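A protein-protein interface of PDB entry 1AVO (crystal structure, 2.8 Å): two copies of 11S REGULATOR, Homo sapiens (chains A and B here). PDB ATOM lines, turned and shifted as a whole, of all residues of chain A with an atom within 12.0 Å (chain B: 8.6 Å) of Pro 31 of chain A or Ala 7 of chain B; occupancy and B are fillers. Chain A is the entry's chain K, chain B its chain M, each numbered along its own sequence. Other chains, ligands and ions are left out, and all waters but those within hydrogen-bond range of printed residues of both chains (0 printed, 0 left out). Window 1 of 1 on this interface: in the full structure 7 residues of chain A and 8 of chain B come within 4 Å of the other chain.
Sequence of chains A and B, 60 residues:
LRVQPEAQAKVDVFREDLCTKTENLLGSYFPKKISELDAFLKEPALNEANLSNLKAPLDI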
ATOM      1  N   THR A  20     -12.361   9.542  -2.581  1.00  0.00           N
ATOM      2  CA  THR A  20     -11.782   8.403  -3.259  1.00  0.00           C
ATOM      3  C   THR A  20     -10.574   8.850  -4.073  1.00  0.00           C
ATOM      4  O   THR A  20      -9.485   8.304  -3.867  1.00  0.00           O
ATOM      5  CB  THR A  20     -12.834   7.791  -4.180  1.00  0.00           C
ATOM      6  OG1 THR A  20     -13.765   7.042  -3.389  1.00  0.00           O
ATOM      7  CG2 THR A  20     -12.204   6.919  -5.231  1.00  0.00           C
ATOM      8  N   LYS A  21     -10.753   9.845  -4.963  1.00  0.00           N
ATOM      9  CA  LYS A  21      -9.644  10.327  -5.779  1.00  0.00           C
ATOM     10  C   LYS A  21      -8.495  10.679  -4.879  1.00  0.00           C
ATOM     11  O   LYS A  21      -7.357  10.401  -5.200  1.00  0.00           O
ATOM     12  CB  LYS A  21      -9.994  11.567  -6.576  1.00  0.00           C
ATOM     13  CG  LYS A  21     -10.911  11.336  -7.727  1.00  0.00           C
ATOM     14  CD  LYS A  21     -11.258  12.699  -8.452  1.00  0.00           C
ATOM     15  CE  LYS A  21     -12.790  12.895  -8.881  1.00  0.00           C
ATOM     16  NZ  LYS A  21     -13.166  14.338  -9.261  1.00  0.00           N
ATOM     17  N   THR A  22      -8.801  11.250  -3.726  1.00  0.00           N
ATOM     18  CA  THR A  22      -7.758  11.635  -2.809  1.00  0.00           C
ATOM     19  C   THR A  22      -7.077  10.530  -2.066  1.00  0.00           C
ATOM     20  O   THR A  22      -5.916  10.653  -1.753  1.00  0.00           O
ATOM     21  CB  THR A  22      -8.247  12.654  -1.811  1.00  0.00           C
ATOM     22  OG1 THR A  22      -8.646  13.819  -2.523  1.00  0.00           O
ATOM     23  CG2 THR A  22      -7.149  13.013  -0.814  1.00  0.00           C
ATOM     24  N   GLU A  23      -7.774   9.469  -1.721  1.00  0.00           N
ATOM     25  CA  GLU A  23      -7.105   8.404  -0.985  1.00  0.00           C
ATOM     26  C   GLU A  23      -6.130   7.798  -1.960  1.00  0.00           C
ATOM     27  O   GLU A  23      -5.048   7.352  -1.563  1.00  0.00           O
ATOM     28  CB  GLU A  23      -8.063   7.300  -0.570  1.00  0.00           C
ATOM     29  CG  GLU A  23      -9.280   7.706   0.261  1.00  0.00           C
ATOM     30  CD  GLU A  23     -10.391   6.618   0.230  1.00  0.00           C
ATOM     31  OE1 GLU A  23     -10.388   5.749  -0.694  1.00  0.00           O
ATOM     32  OE2 GLU A  23     -11.272   6.636   1.129  1.00  0.00           O
ATOM     33  N   ASN A  24      -6.529   7.788  -3.233  1.00  0.00           N
ATOM     34  CA  ASN A  24      -5.714   7.227  -4.310  1.00  0.00           C
ATOM     35  C   ASN A  24      -4.497   8.075  -4.632  1.00  0.00           C
ATOM     36  O   ASN A  24      -3.428   7.554  -4.911  1.00  0.00           O
ATOM     37  CB  ASN A  24      -6.539   7.011  -5.581  1.00  0.00           C
ATOM     38  CG  ASN A  24      -7.684   6.005  -5.390  1.00  0.00           C
ATOM     39  OD1 ASN A  24      -7.678   5.183  -4.452  1.00  0.00           O
ATOM     40  ND2 ASN A  24      -8.672   6.066  -6.290  1.00  0.00           N
ATOM     41  N   LEU A  25      -4.672   9.389  -4.652  1.00  0.00           N
ATOM     42  CA  LEU A  25      -3.577  10.309  -4.889  1.00  0.00           C
ATOM     43  C   LEU A  25      -2.483  10.044  -3.863  1.00  0.00           C
ATOM     44  O   LEU A  25      -1.348   9.754  -4.212  1.00  0.00           O
ATOM     45  CB  LEU A  25      -4.091  11.706  -4.667  1.00  0.00           C
ATOM     46  CG  LEU A  25      -4.099  12.641  -5.848  1.00  0.00           C
ATOM     47  CD1 LEU A  25      -4.557  11.919  -7.096  1.00  0.00           C
ATOM     48  CD2 LEU A  25      -5.006  13.796  -5.500  1.00  0.00           C
ATOM     49  N   LEU A  26      -2.839  10.118  -2.589  1.00  0.00           N
ATOM     50  CA  LEU A  26      -1.866   9.898  -1.526  1.00  0.00           C
ATOM     51  C   LEU A  26      -1.260   8.501  -1.505  1.00  0.00           C
ATOM     52  O   LEU A  26      -0.043   8.340  -1.567  1.00  0.00           O
ATOM     53  CB  LEU A  26      -2.471  10.256  -0.154  1.00  0.00           C
ATOM     54  CG  LEU A  26      -3.120  11.652  -0.196  1.00  0.00           C
ATOM     55  CD1 LEU A  26      -3.957  11.923   1.048  1.00  0.00           C
ATOM     56  CD2 LEU A  26      -2.056  12.736  -0.441  1.00  0.00           C
ATOM     57  N   GLY A  27      -2.110   7.490  -1.462  1.00  0.00           N
ATOM     58  CA  GLY A  27      -1.615   6.131  -1.416  1.00  0.00           C
ATOM     59  C   GLY A  27      -0.922   5.553  -2.631  1.00  0.00           C
ATOM     60  O   GLY A  27      -0.289   4.516  -2.506  1.00  0.00           O
ATOM     61  N   SER A  28      -0.986   6.217  -3.780  1.00  0.00           N
ATOM     62  CA  SER A  28      -0.368   5.676  -5.009  1.00  0.00           C
ATOM     63  C   SER A  28       0.213   6.606  -6.120  1.00  0.00           C
ATOM     64  O   SER A  28       1.323   6.382  -6.614  1.00  0.00           O
ATOM     65  CB  SER A  28      -1.358   4.722  -5.677  1.00  0.00           C
ATOM     66  OG  SER A  28      -1.425   4.950  -7.094  1.00  0.00           O
ATOM     67  N   TYR A  29      -0.612   7.533  -6.603  1.00  0.00           N
ATOM     68  CA  TYR A  29      -0.252   8.473  -7.652  1.00  0.00           C
ATOM     69  C   TYR A  29       0.955   9.295  -7.281  1.00  0.00           C
ATOM     70  O   TYR A  29       1.879   9.424  -8.080  1.00  0.00           O
ATOM     71  CB  TYR A  29      -1.407   9.411  -7.865  1.00  0.00           C
ATOM     72  CG  TYR A  29      -1.291  10.202  -9.092  1.00  0.00           C
ATOM     73  CD1 TYR A  29      -1.794   9.734 -10.279  1.00  0.00           C
ATOM     74  CD2 TYR A  29      -0.728  11.454  -9.065  1.00  0.00           C
ATOM     75  CE1 TYR A  29      -1.745  10.494 -11.410  1.00  0.00           C
ATOM     76  CE2 TYR A  29      -0.674  12.239 -10.202  1.00  0.00           C
ATOM     77  CZ  TYR A  29      -1.187  11.748 -11.378  1.00  0.00           C
ATOM     78  OH  TYR A  29      -1.139  12.516 -12.532  1.00  0.00           O
ATOM     79  N   PHE A  30       0.914   9.905  -6.095  1.00  0.00           N
ATOM     80  CA  PHE A  30       2.024  10.717  -5.620  1.00  0.00           C
ATOM     81  C   PHE A  30       3.330   9.929  -5.531  1.00  0.00           C
ATOM     82  O   PHE A  30       4.338  10.394  -6.064  1.00  0.00           O
ATOM     83  CB  PHE A  30       1.698  11.414  -4.302  1.00  0.00           C
ATOM     84  CG  PHE A  30       0.805  12.627  -4.450  1.00  0.00           C
ATOM     85  CD1 PHE A  30       0.096  12.858  -5.635  1.00  0.00           C
ATOM     86  CD2 PHE A  30       0.654  13.531  -3.399  1.00  0.00           C
ATOM     87  CE1 PHE A  30      -0.749  13.962  -5.778  1.00  0.00           C
ATOM     88  CE2 PHE A  30      -0.203  14.647  -3.538  1.00  0.00           C
ATOM     89  CZ  PHE A  30      -0.898  14.851  -4.730  1.00  0.00           C
ATOM     90  N   PRO A  31       3.358   8.747  -4.854  1.00  0.00           N
ATOM     91  CA  PRO A  31       4.600   7.950  -4.763  1.00  0.00           C
ATOM     92  C   PRO A  31       5.090   7.529  -6.153  1.00  0.00           C
ATOM     93  O   PRO A  31       6.283   7.442  -6.420  1.00  0.00           O
ATOM     94  CB  PRO A  31       4.162   6.740  -3.967  1.00  0.00           C
ATOM     95  CG  PRO A  31       3.126   7.314  -3.040  1.00  0.00           C
ATOM     96  CD  PRO A  31       2.316   8.161  -3.988  1.00  0.00           C
ATOM     97  N   LYS A  32       4.145   7.345  -7.058  1.00  0.00           N
ATOM     98  CA  LYS A  32       4.439   6.965  -8.428  1.00  0.00           C
ATOM     99  C   LYS A  32       5.103   8.118  -9.174  1.00  0.00           C
ATOM    100  O   LYS A  32       6.160   7.948  -9.778  1.00  0.00           O
ATOM    101  CB  LYS A  32       3.145   6.556  -9.131  1.00  0.00           C
ATOM    102  CG  LYS A  32       3.232   6.469 -10.663  1.00  0.00           C
ATOM    103  CD  LYS A  32       1.834   6.687 -11.325  1.00  0.00           C
ATOM    104  CE  LYS A  32       0.755   5.759 -10.688  1.00  0.00           C
ATOM    105  NZ  LYS A  32      -0.711   6.145 -10.932  1.00  0.00           N
ATOM    106  N   LYS A  33       4.475   9.294  -9.139  1.00  0.00           N
ATOM    107  CA  LYS A  33       5.011  10.455  -9.832  1.00  0.00           C
ATOM    108  C   LYS A  33       6.392  10.866  -9.337  1.00  0.00           C
ATOM    109  O   LYS A  33       7.209  11.335 -10.104  1.00  0.00           O
ATOM    110  CB  LYS A  33       4.053  11.586  -9.675  1.00  0.00           C
ATOM    111  CG  LYS A  33       2.904  11.419 -10.521  1.00  0.00           C
ATOM    112  CD  LYS A  33       3.379  11.664 -11.882  1.00  0.00           C
ATOM    113  CE  LYS A  33       2.227  11.851 -12.841  1.00  0.00           C
ATOM    114  NZ  LYS A  33       2.733  11.837 -14.259  1.00  0.00           N
ATOM    115  N   ILE A  34       6.619  10.730  -8.032  1.00  0.00           N
ATOM    116  CA  ILE A  34       7.887  11.089  -7.416  1.00  0.00           C
ATOM    117  C   ILE A  34       8.951  10.193  -7.994  1.00  0.00           C
ATOM    118  O   ILE A  34      10.078  10.581  -8.167  1.00  0.00           O
ATOM    119  CB  ILE A  34       7.830  10.875  -5.931  1.00  0.00           C
ATOM    120  CG1 ILE A  34       6.985  11.972  -5.282  1.00  0.00           C
ATOM    121  CG2 ILE A  34       9.218  10.806  -5.363  1.00  0.00           C
ATOM    122  CD1 ILE A  34       6.589  11.600  -3.847  1.00  0.00           C
ATOM    123  N   SER A  35       8.605   8.950  -8.228  1.00  0.00           N
ATOM    124  CA  SER A  35       9.565   8.039  -8.811  1.00  0.00           C
ATOM    125  C   SER A  35       9.782   8.279 -10.278  1.00  0.00           C
ATOM    126  O   SER A  35      10.906   8.226 -10.745  1.00  0.00           O
ATOM    127  CB  SER A  35       9.139   6.605  -8.600  1.00  0.00           C
ATOM    128  OG  SER A  35       9.316   6.300  -7.232  1.00  0.00           O
ATOM    129  N   GLU A  36       8.715   8.525 -11.023  1.00  0.00           N
ATOM    130  CA  GLU A  36       8.849   8.769 -12.467  1.00  0.00           C
ATOM    131  C   GLU A  36       9.737   9.963 -12.775  1.00  0.00           C
ATOM    132  O   GLU A  36      10.692   9.861 -13.518  1.00  0.00           O
ATOM    133  CB  GLU A  36       7.474   8.995 -13.098  1.00  0.00           C
ATOM    134  CG  GLU A  36       6.444   7.875 -12.811  1.00  0.00           C
ATOM    135  CD  GLU A  36       5.112   8.034 -13.583  1.00  0.00           C
ATOM    136  OE1 GLU A  36       4.783   9.154 -14.080  1.00  0.00           O
ATOM    137  OE2 GLU A  36       4.391   7.015 -13.694  1.00  0.00           O
ATOM    138  N   LEU A  37       9.399  11.095 -12.193  1.00  0.00           N
ATOM    139  CA  LEU A  37      10.147  12.329 -12.394  1.00  0.00           C
ATOM    140  C   LEU A  37      11.580  12.198 -11.919  1.00  0.00           C
ATOM    141  O   LEU A  37      12.495  12.724 -12.540  1.00  0.00           O
ATOM    142  CB  LEU A  37       9.461  13.480 -11.644  1.00  0.00           C
ATOM    143  CG  LEU A  37       8.030  13.734 -12.100  1.00  0.00           C
ATOM    144  CD1 LEU A  37       7.243  14.443 -11.053  1.00  0.00           C
ATOM    145  CD2 LEU A  37       8.086  14.527 -13.382  1.00  0.00           C
ATOM    146  N   ASP A  38      11.771  11.494 -10.812  1.00  0.00           N
ATOM    147  CA  ASP A  38      13.109  11.316 -10.268  1.00  0.00           C
ATOM    148  C   ASP A  38      13.962  10.587 -11.295  1.00  0.00           C
ATOM    149  O   ASP A  38      15.144  10.873 -11.444  1.00  0.00           O
ATOM    150  CB  ASP A  38      13.062  10.561  -8.942  1.00  0.00           C
ATOM    151  CG  ASP A  38      14.321  10.768  -8.103  1.00  0.00           C
ATOM    152  OD1 ASP A  38      15.091  11.719  -8.390  1.00  0.00           O
ATOM    153  OD2 ASP A  38      14.551   9.983  -7.143  1.00  0.00           O
ATOM    154  N   ALA A  39      13.337   9.693 -12.050  1.00  0.00           N
ATOM    155  CA  ALA A  39      14.023   8.952 -13.087  1.00  0.00           C
ATOM    156  C   ALA A  39      14.321   9.837 -14.295  1.00  0.00           C
ATOM    157  O   ALA A  39      15.409   9.795 -14.856  1.00  0.00           O
ATOM    158  CB  ALA A  39      13.179   7.826 -13.507  1.00  0.00           C
ATOM    159  N   PHE A  40      13.330  10.629 -14.692  1.00  0.00           N
ATOM    160  CA  PHE A  40      13.442  11.543 -15.819  1.00  0.00           C
ATOM    161  C   PHE A  40      14.667  12.399 -15.623  1.00  0.00           C
ATOM    162  O   PHE A  40      15.440  12.611 -16.540  1.00  0.00           O
ATOM    163  CB  PHE A  40      12.193  12.433 -15.861  1.00  0.00           C
ATOM    164  CG  PHE A  40      12.085  13.322 -17.088  1.00  0.00           C
ATOM    165  CD1 PHE A  40      12.964  13.212 -18.138  1.00  0.00           C
ATOM    166  CD2 PHE A  40      11.101  14.295 -17.164  1.00  0.00           C
ATOM    167  CE1 PHE A  40      12.864  14.061 -19.239  1.00  0.00           C
ATOM    168  CE2 PHE A  40      11.010  15.140 -18.265  1.00  0.00           C
ATOM    169  CZ  PHE A  40      11.892  15.017 -19.299  1.00  0.00           C
ATOM    170  N   ARG B   2      -4.581   4.501   3.486  1.00  0.00           N
ATOM    171  CA  ARG B   2      -3.896   3.296   3.020  1.00  0.00           C
ATOM    172  C   ARG B   2      -2.821   3.554   1.965  1.00  0.00           C
ATOM    173  O   ARG B   2      -3.138   3.836   0.787  1.00  0.00           O
ATOM    174  CB  ARG B   2      -4.903   2.304   2.426  1.00  0.00           C
ATOM    175  CG  ARG B   2      -6.008   1.857   3.365  1.00  0.00           C
ATOM    176  CD  ARG B   2      -7.116   1.145   2.586  1.00  0.00           C
ATOM    177  NE  ARG B   2      -8.241   0.770   3.444  1.00  0.00           N
ATOM    178  CZ  ARG B   2      -9.498   0.582   3.027  1.00  0.00           C
ATOM    179  NH1 ARG B   2      -9.824   0.732   1.739  1.00  0.00           N
ATOM    180  NH2 ARG B   2     -10.440   0.236   3.907  1.00  0.00           N
ATOM    181  N   VAL B   3      -1.557   3.503   2.381  1.00  0.00           N
ATOM    182  CA  VAL B   3      -0.481   3.659   1.413  1.00  0.00           C
ATOM    183  C   VAL B   3       0.130   2.287   1.211  1.00  0.00           C
ATOM    184  O   VAL B   3       0.636   1.641   2.133  1.00  0.00           O
ATOM    185  CB  VAL B   3       0.588   4.709   1.789  1.00  0.00           C
ATOM    186  CG1 VAL B   3       1.563   4.912   0.608  1.00  0.00           C
ATOM    187  CG2 VAL B   3      -0.092   6.023   2.138  1.00  0.00           C
ATOM    188  N   GLN B   4      -0.064   1.822  -0.006  1.00  0.00           N
ATOM    189  CA  GLN B   4       0.418   0.546  -0.462  1.00  0.00           C
ATOM    190  C   GLN B   4       1.914   0.396  -0.185  1.00  0.00           C
ATOM    191  O   GLN B   4       2.670   1.361  -0.351  1.00  0.00           O
ATOM    192  CB  GLN B   4       0.142   0.466  -1.963  1.00  0.00           C
ATOM    193  CG  GLN B   4      -1.345   0.581  -2.282  1.00  0.00           C
ATOM    194  CD  GLN B   4      -2.171  -0.462  -1.501  1.00  0.00           C
ATOM    195  OE1 GLN B   4      -1.758  -1.633  -1.362  1.00  0.00           O
ATOM    196  NE2 GLN B   4      -3.333  -0.037  -0.975  1.00  0.00           N
ATOM    197  N   PRO B   5       2.364  -0.818   0.221  1.00  0.00           N
ATOM    198  CA  PRO B   5       3.784  -1.094   0.520  1.00  0.00           C
ATOM    199  C   PRO B   5       4.806  -0.743  -0.600  1.00  0.00           C
ATOM    200  O   PRO B   5       5.899  -0.237  -0.326  1.00  0.00           O
ATOM    201  CB  PRO B   5       3.771  -2.585   0.890  1.00  0.00           C
ATOM    202  CG  PRO B   5       2.582  -3.124   0.120  1.00  0.00           C
ATOM    203  CD  PRO B   5       1.557  -2.042   0.396  1.00  0.00           C
ATOM    204  N   GLU B   6       4.470  -1.012  -1.853  1.00  0.00           N
ATOM    205  CA  GLU B   6       5.374  -0.665  -2.947  1.00  0.00           C
ATOM    206  C   GLU B   6       5.384   0.863  -3.167  1.00  0.00           C
ATOM    207  O   GLU B   6       6.331   1.418  -3.719  1.00  0.00           O
ATOM    208  CB  GLU B   6       4.921  -1.349  -4.246  1.00  0.00           C
ATOM    209  CG  GLU B   6       3.690  -0.684  -4.992  1.00  0.00           C
ATOM    210  CD  GLU B   6       2.279  -1.208  -4.564  1.00  0.00           C
ATOM    211  OE1 GLU B   6       2.020  -1.359  -3.344  1.00  0.00           O
ATOM    212  OE2 GLU B   6       1.423  -1.453  -5.456  1.00  0.00           O
ATOM    213  N   ALA B   7       4.296   1.522  -2.778  1.00  0.00           N
ATOM    214  CA  ALA B   7       4.163   2.950  -2.954  1.00  0.00           C
ATOM    215  C   ALA B   7       4.937   3.638  -1.874  1.00  0.00           C
ATOM    216  O   ALA B   7       5.641   4.587  -2.135  1.00  0.00           O
ATOM    217  CB  ALA B   7       2.732   3.347  -2.878  1.00  0.00           C
ATOM    218  N   GLN B   8       4.807   3.164  -0.648  1.00  0.00           N
ATOM    219  CA  GLN B   8       5.547   3.780   0.443  1.00  0.00           C
ATOM    220  C   GLN B   8       7.006   3.581   0.151  1.00  0.00           C
ATOM    221  O   GLN B   8       7.803   4.467   0.377  1.00  0.00           O
ATOM    222  CB  GLN B   8       5.203   3.160   1.801  1.00  0.00           C
ATOM    223  CG  GLN B   8       6.008   3.725   2.983  1.00  0.00           C
ATOM    224  CD  GLN B   8       5.861   5.257   3.162  1.00  0.00           C
ATOM    225  OE1 GLN B   8       4.972   5.753   3.886  1.00  0.00           O
ATOM    226  NE2 GLN B   8       6.754   6.004   2.519  1.00  0.00           N
ATOM    227  N   ALA B   9       7.341   2.441  -0.431  1.00  0.00           N
ATOM    228  CA  ALA B   9       8.721   2.136  -0.754  1.00  0.00           C
ATOM    229  C   ALA B   9       9.322   3.113  -1.736  1.00  0.00           C
ATOM    230  O   ALA B   9      10.466   3.494  -1.582  1.00  0.00           O
ATOM    231  CB  ALA B   9       8.825   0.788  -1.285  1.00  0.00           C
ATOM    232  N   LYS B  10       8.566   3.498  -2.762  1.00  0.00           N
ATOM    233  CA  LYS B  10       9.038   4.494  -3.758  1.00  0.00           C
ATOM    234  C   LYS B  10       9.492   5.780  -3.044  1.00  0.00           C
ATOM    235  O   LYS B  10      10.553   6.329  -3.348  1.00  0.00           O
ATOM    236  CB  LYS B  10       7.918   4.840  -4.758  1.00  0.00           C
ATOM    237  CG  LYS B  10       7.674   3.765  -5.818  1.00  0.00           C
ATOM    238  CD  LYS B  10       6.223   3.764  -6.274  1.00  0.00           C
ATOM    239  CE  LYS B  10       5.969   2.781  -7.399  1.00  0.00           C
ATOM    240  NZ  LYS B  10       6.579   3.215  -8.695  1.00  0.00           N
ATOM    241  N   VAL B  11       8.681   6.207  -2.075  1.00  0.00           N
ATOM    242  CA  VAL B  11       8.912   7.391  -1.269  1.00  0.00           C
ATOM    243  C   VAL B  11      10.119   7.230  -0.372  1.00  0.00           C
ATOM    244  O   VAL B  11      10.982   8.107  -0.322  1.00  0.00           O
ATOM    245  CB  VAL B  11       7.719   7.666  -0.376  1.00  0.00           C
ATOM    246  CG1 VAL B  11       8.018   8.843   0.468  1.00  0.00           C
ATOM    247  CG2 VAL B  11       6.466   7.884  -1.203  1.00  0.00           C
ATOM    248  N   ASP B  12      10.170   6.119   0.352  1.00  0.00           N
ATOM    249  CA  ASP B  12      11.282   5.865   1.257  1.00  0.00           C
ATOM    250  C   ASP B  12      12.616   5.997   0.537  1.00  0.00           C
ATOM    251  O   ASP B  12      13.565   6.567   1.085  1.00  0.00           O
ATOM    252  CB  ASP B  12      11.172   4.472   1.866  1.00  0.00           C
ATOM    253  CG  ASP B  12      10.097   4.379   2.955  1.00  0.00           C
ATOM    254  OD1 ASP B  12       9.605   5.444   3.432  1.00  0.00           O
ATOM    255  OD2 ASP B  12       9.752   3.227   3.340  1.00  0.00           O
ATOM    256  N   VAL B  13      12.656   5.486  -0.698  1.00  0.00           N
ATOM    257  CA  VAL B  13      13.841   5.512  -1.538  1.00  0.00           C
ATOM    258  C   VAL B  13      14.196   6.930  -1.874  1.00  0.00           C
ATOM    259  O   VAL B  13      15.342   7.313  -1.766  1.00  0.00           O
ATOM    260  CB  VAL B  13      13.644   4.753  -2.848  1.00  0.00           C
ATOM    261  CG1 VAL B  13      14.812   4.962  -3.734  1.00  0.00           C
ATOM    262  CG2 VAL B  13      13.506   3.269  -2.583  1.00  0.00           C
ATOM    263  N   PHE B  14      13.228   7.726  -2.290  1.00  0.00           N
ATOM    264  CA  PHE B  14      13.512   9.114  -2.603  1.00  0.00           C
ATOM    265  C   PHE B  14      14.068   9.818  -1.370  1.00  0.00           C
ATOM    266  O   PHE B  14      15.066  10.529  -1.436  1.00  0.00           O
ATOM    267  CB  PHE B  14      12.237   9.821  -3.016  1.00  0.00           C
ATOM    268  CG  PHE B  14      12.376  11.323  -3.119  1.00  0.00           C
ATOM    269  CD1 PHE B  14      13.174  11.887  -4.099  1.00  0.00           C
ATOM    270  CD2 PHE B  14      11.679  12.178  -2.255  1.00  0.00           C
ATOM    271  CE1 PHE B  14      13.277  13.286  -4.226  1.00  0.00           C
ATOM    272  CE2 PHE B  14      11.782  13.566  -2.379  1.00  0.00           C
ATOM    273  CZ  PHE B  14      12.582  14.110  -3.368  1.00  0.00           C
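The side-chain hydroxyl (OG) of Ser 35 of chain A lies within hydrogen-bond range of the backbone carbonyl oxygen (O) of Pro 31 of chain A (3.3 Å).
Among the printed residues, pairs that only touch across the chains: Pro 31 of chain A with Ala 7 of chain B, Ser 35 of chain A with Lys 10 of chain B, Gly 27 of chain A with Ala 7 of chain B, Pro 31 of chain A with Lys 10 of chain B, Gly 27 of chain A with Arg 2 of chain B, Gly 27 of chain A with Val 3 of chain B, Gly 27 of chain A with Gln 4 of chain B, Pro 31 of chain A with Val 11 of chain B, Asp 38 of chain A with Phe 14 of chain B and Ile 34 of chain A with Phe 14 of chain B.
Of the printed residues of chain B, Gly 27 of chain A touches Arg 2 (3.5 Å), Val 3 (3.6 Å), Gln 4 (3.7 Å) and Ala 7 (3.3 Å). Of chain B, only Ala 7, Lys 10 and Val 11 come within 4 Å of Pro 31 of chain A. Of the printed residues of chain B, Ile 34 of chain A touches Phe 14. Of the printed residues of chain B, Asp 38 of chain A touches Phe 14 (3.8 Å). Printed residues of chain A within 4 Å of Arg 2 of chain B: Gly 27. Val 3 of chain B touches one residue of chain A. Printed residues of chain A within 4 Å of Gln 4 of chain B: Gly 27. No residue of chain A comes within 4 Å of Pro 5 of chain B. Glu 6 of chain B touches none of the printed residues of chain A. Of chain A, only Gly 27 (3.3 Å) and Pro 31 (3.2 Å) come within 4 Å of Ala 7 of chain B. No residue of chain A comes within 4 Å of Ala 9 of chain B. Lys 10 of chain B touches just these residues of chain A: Pro 31 (3.5 Å) and Ser 35 (3.2 Å). Val 11 of chain B touches one residue of chain A. Printed residues of chain A within 4 Å of Phe 14 of chain B: Ile 34 and Asp 38. The nearest residue of chain A that does not touch Ala 7 of chain B is Ser 28 of chain A (4.4 Å). The nearest printed residue of chain A that does not touch Phe 14 of chain B is Ser 35 of chain A (6.2 Å).
Of the 13 printed residues of chain B, 7 touch a printed residue of chain A. Hydrophobic or aromatic side chains of chain B that line the printed part of chain A: Val 3, Ala 7, Val 11 and Phe 14. Of the 21 printed residues of chain A, 5 touch a printed residue of chain B. Hydrophobic or aromatic side chains of chain A within 4 Å of the printed part of chain B: Pro 31 and Ile 34. Along chain A the printed residues that touch a printed residue of chain B span positions 27 to 38. Among the printed residues, no Asp or Glu carboxylate lies within 4 Å of a Lys or Arg side-chain nitrogen of the other chain.
No position is printed for both chains. Of the 10 pairs that touch across the chains among the printed residues, none has its exchanged pair printed and touching as well.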
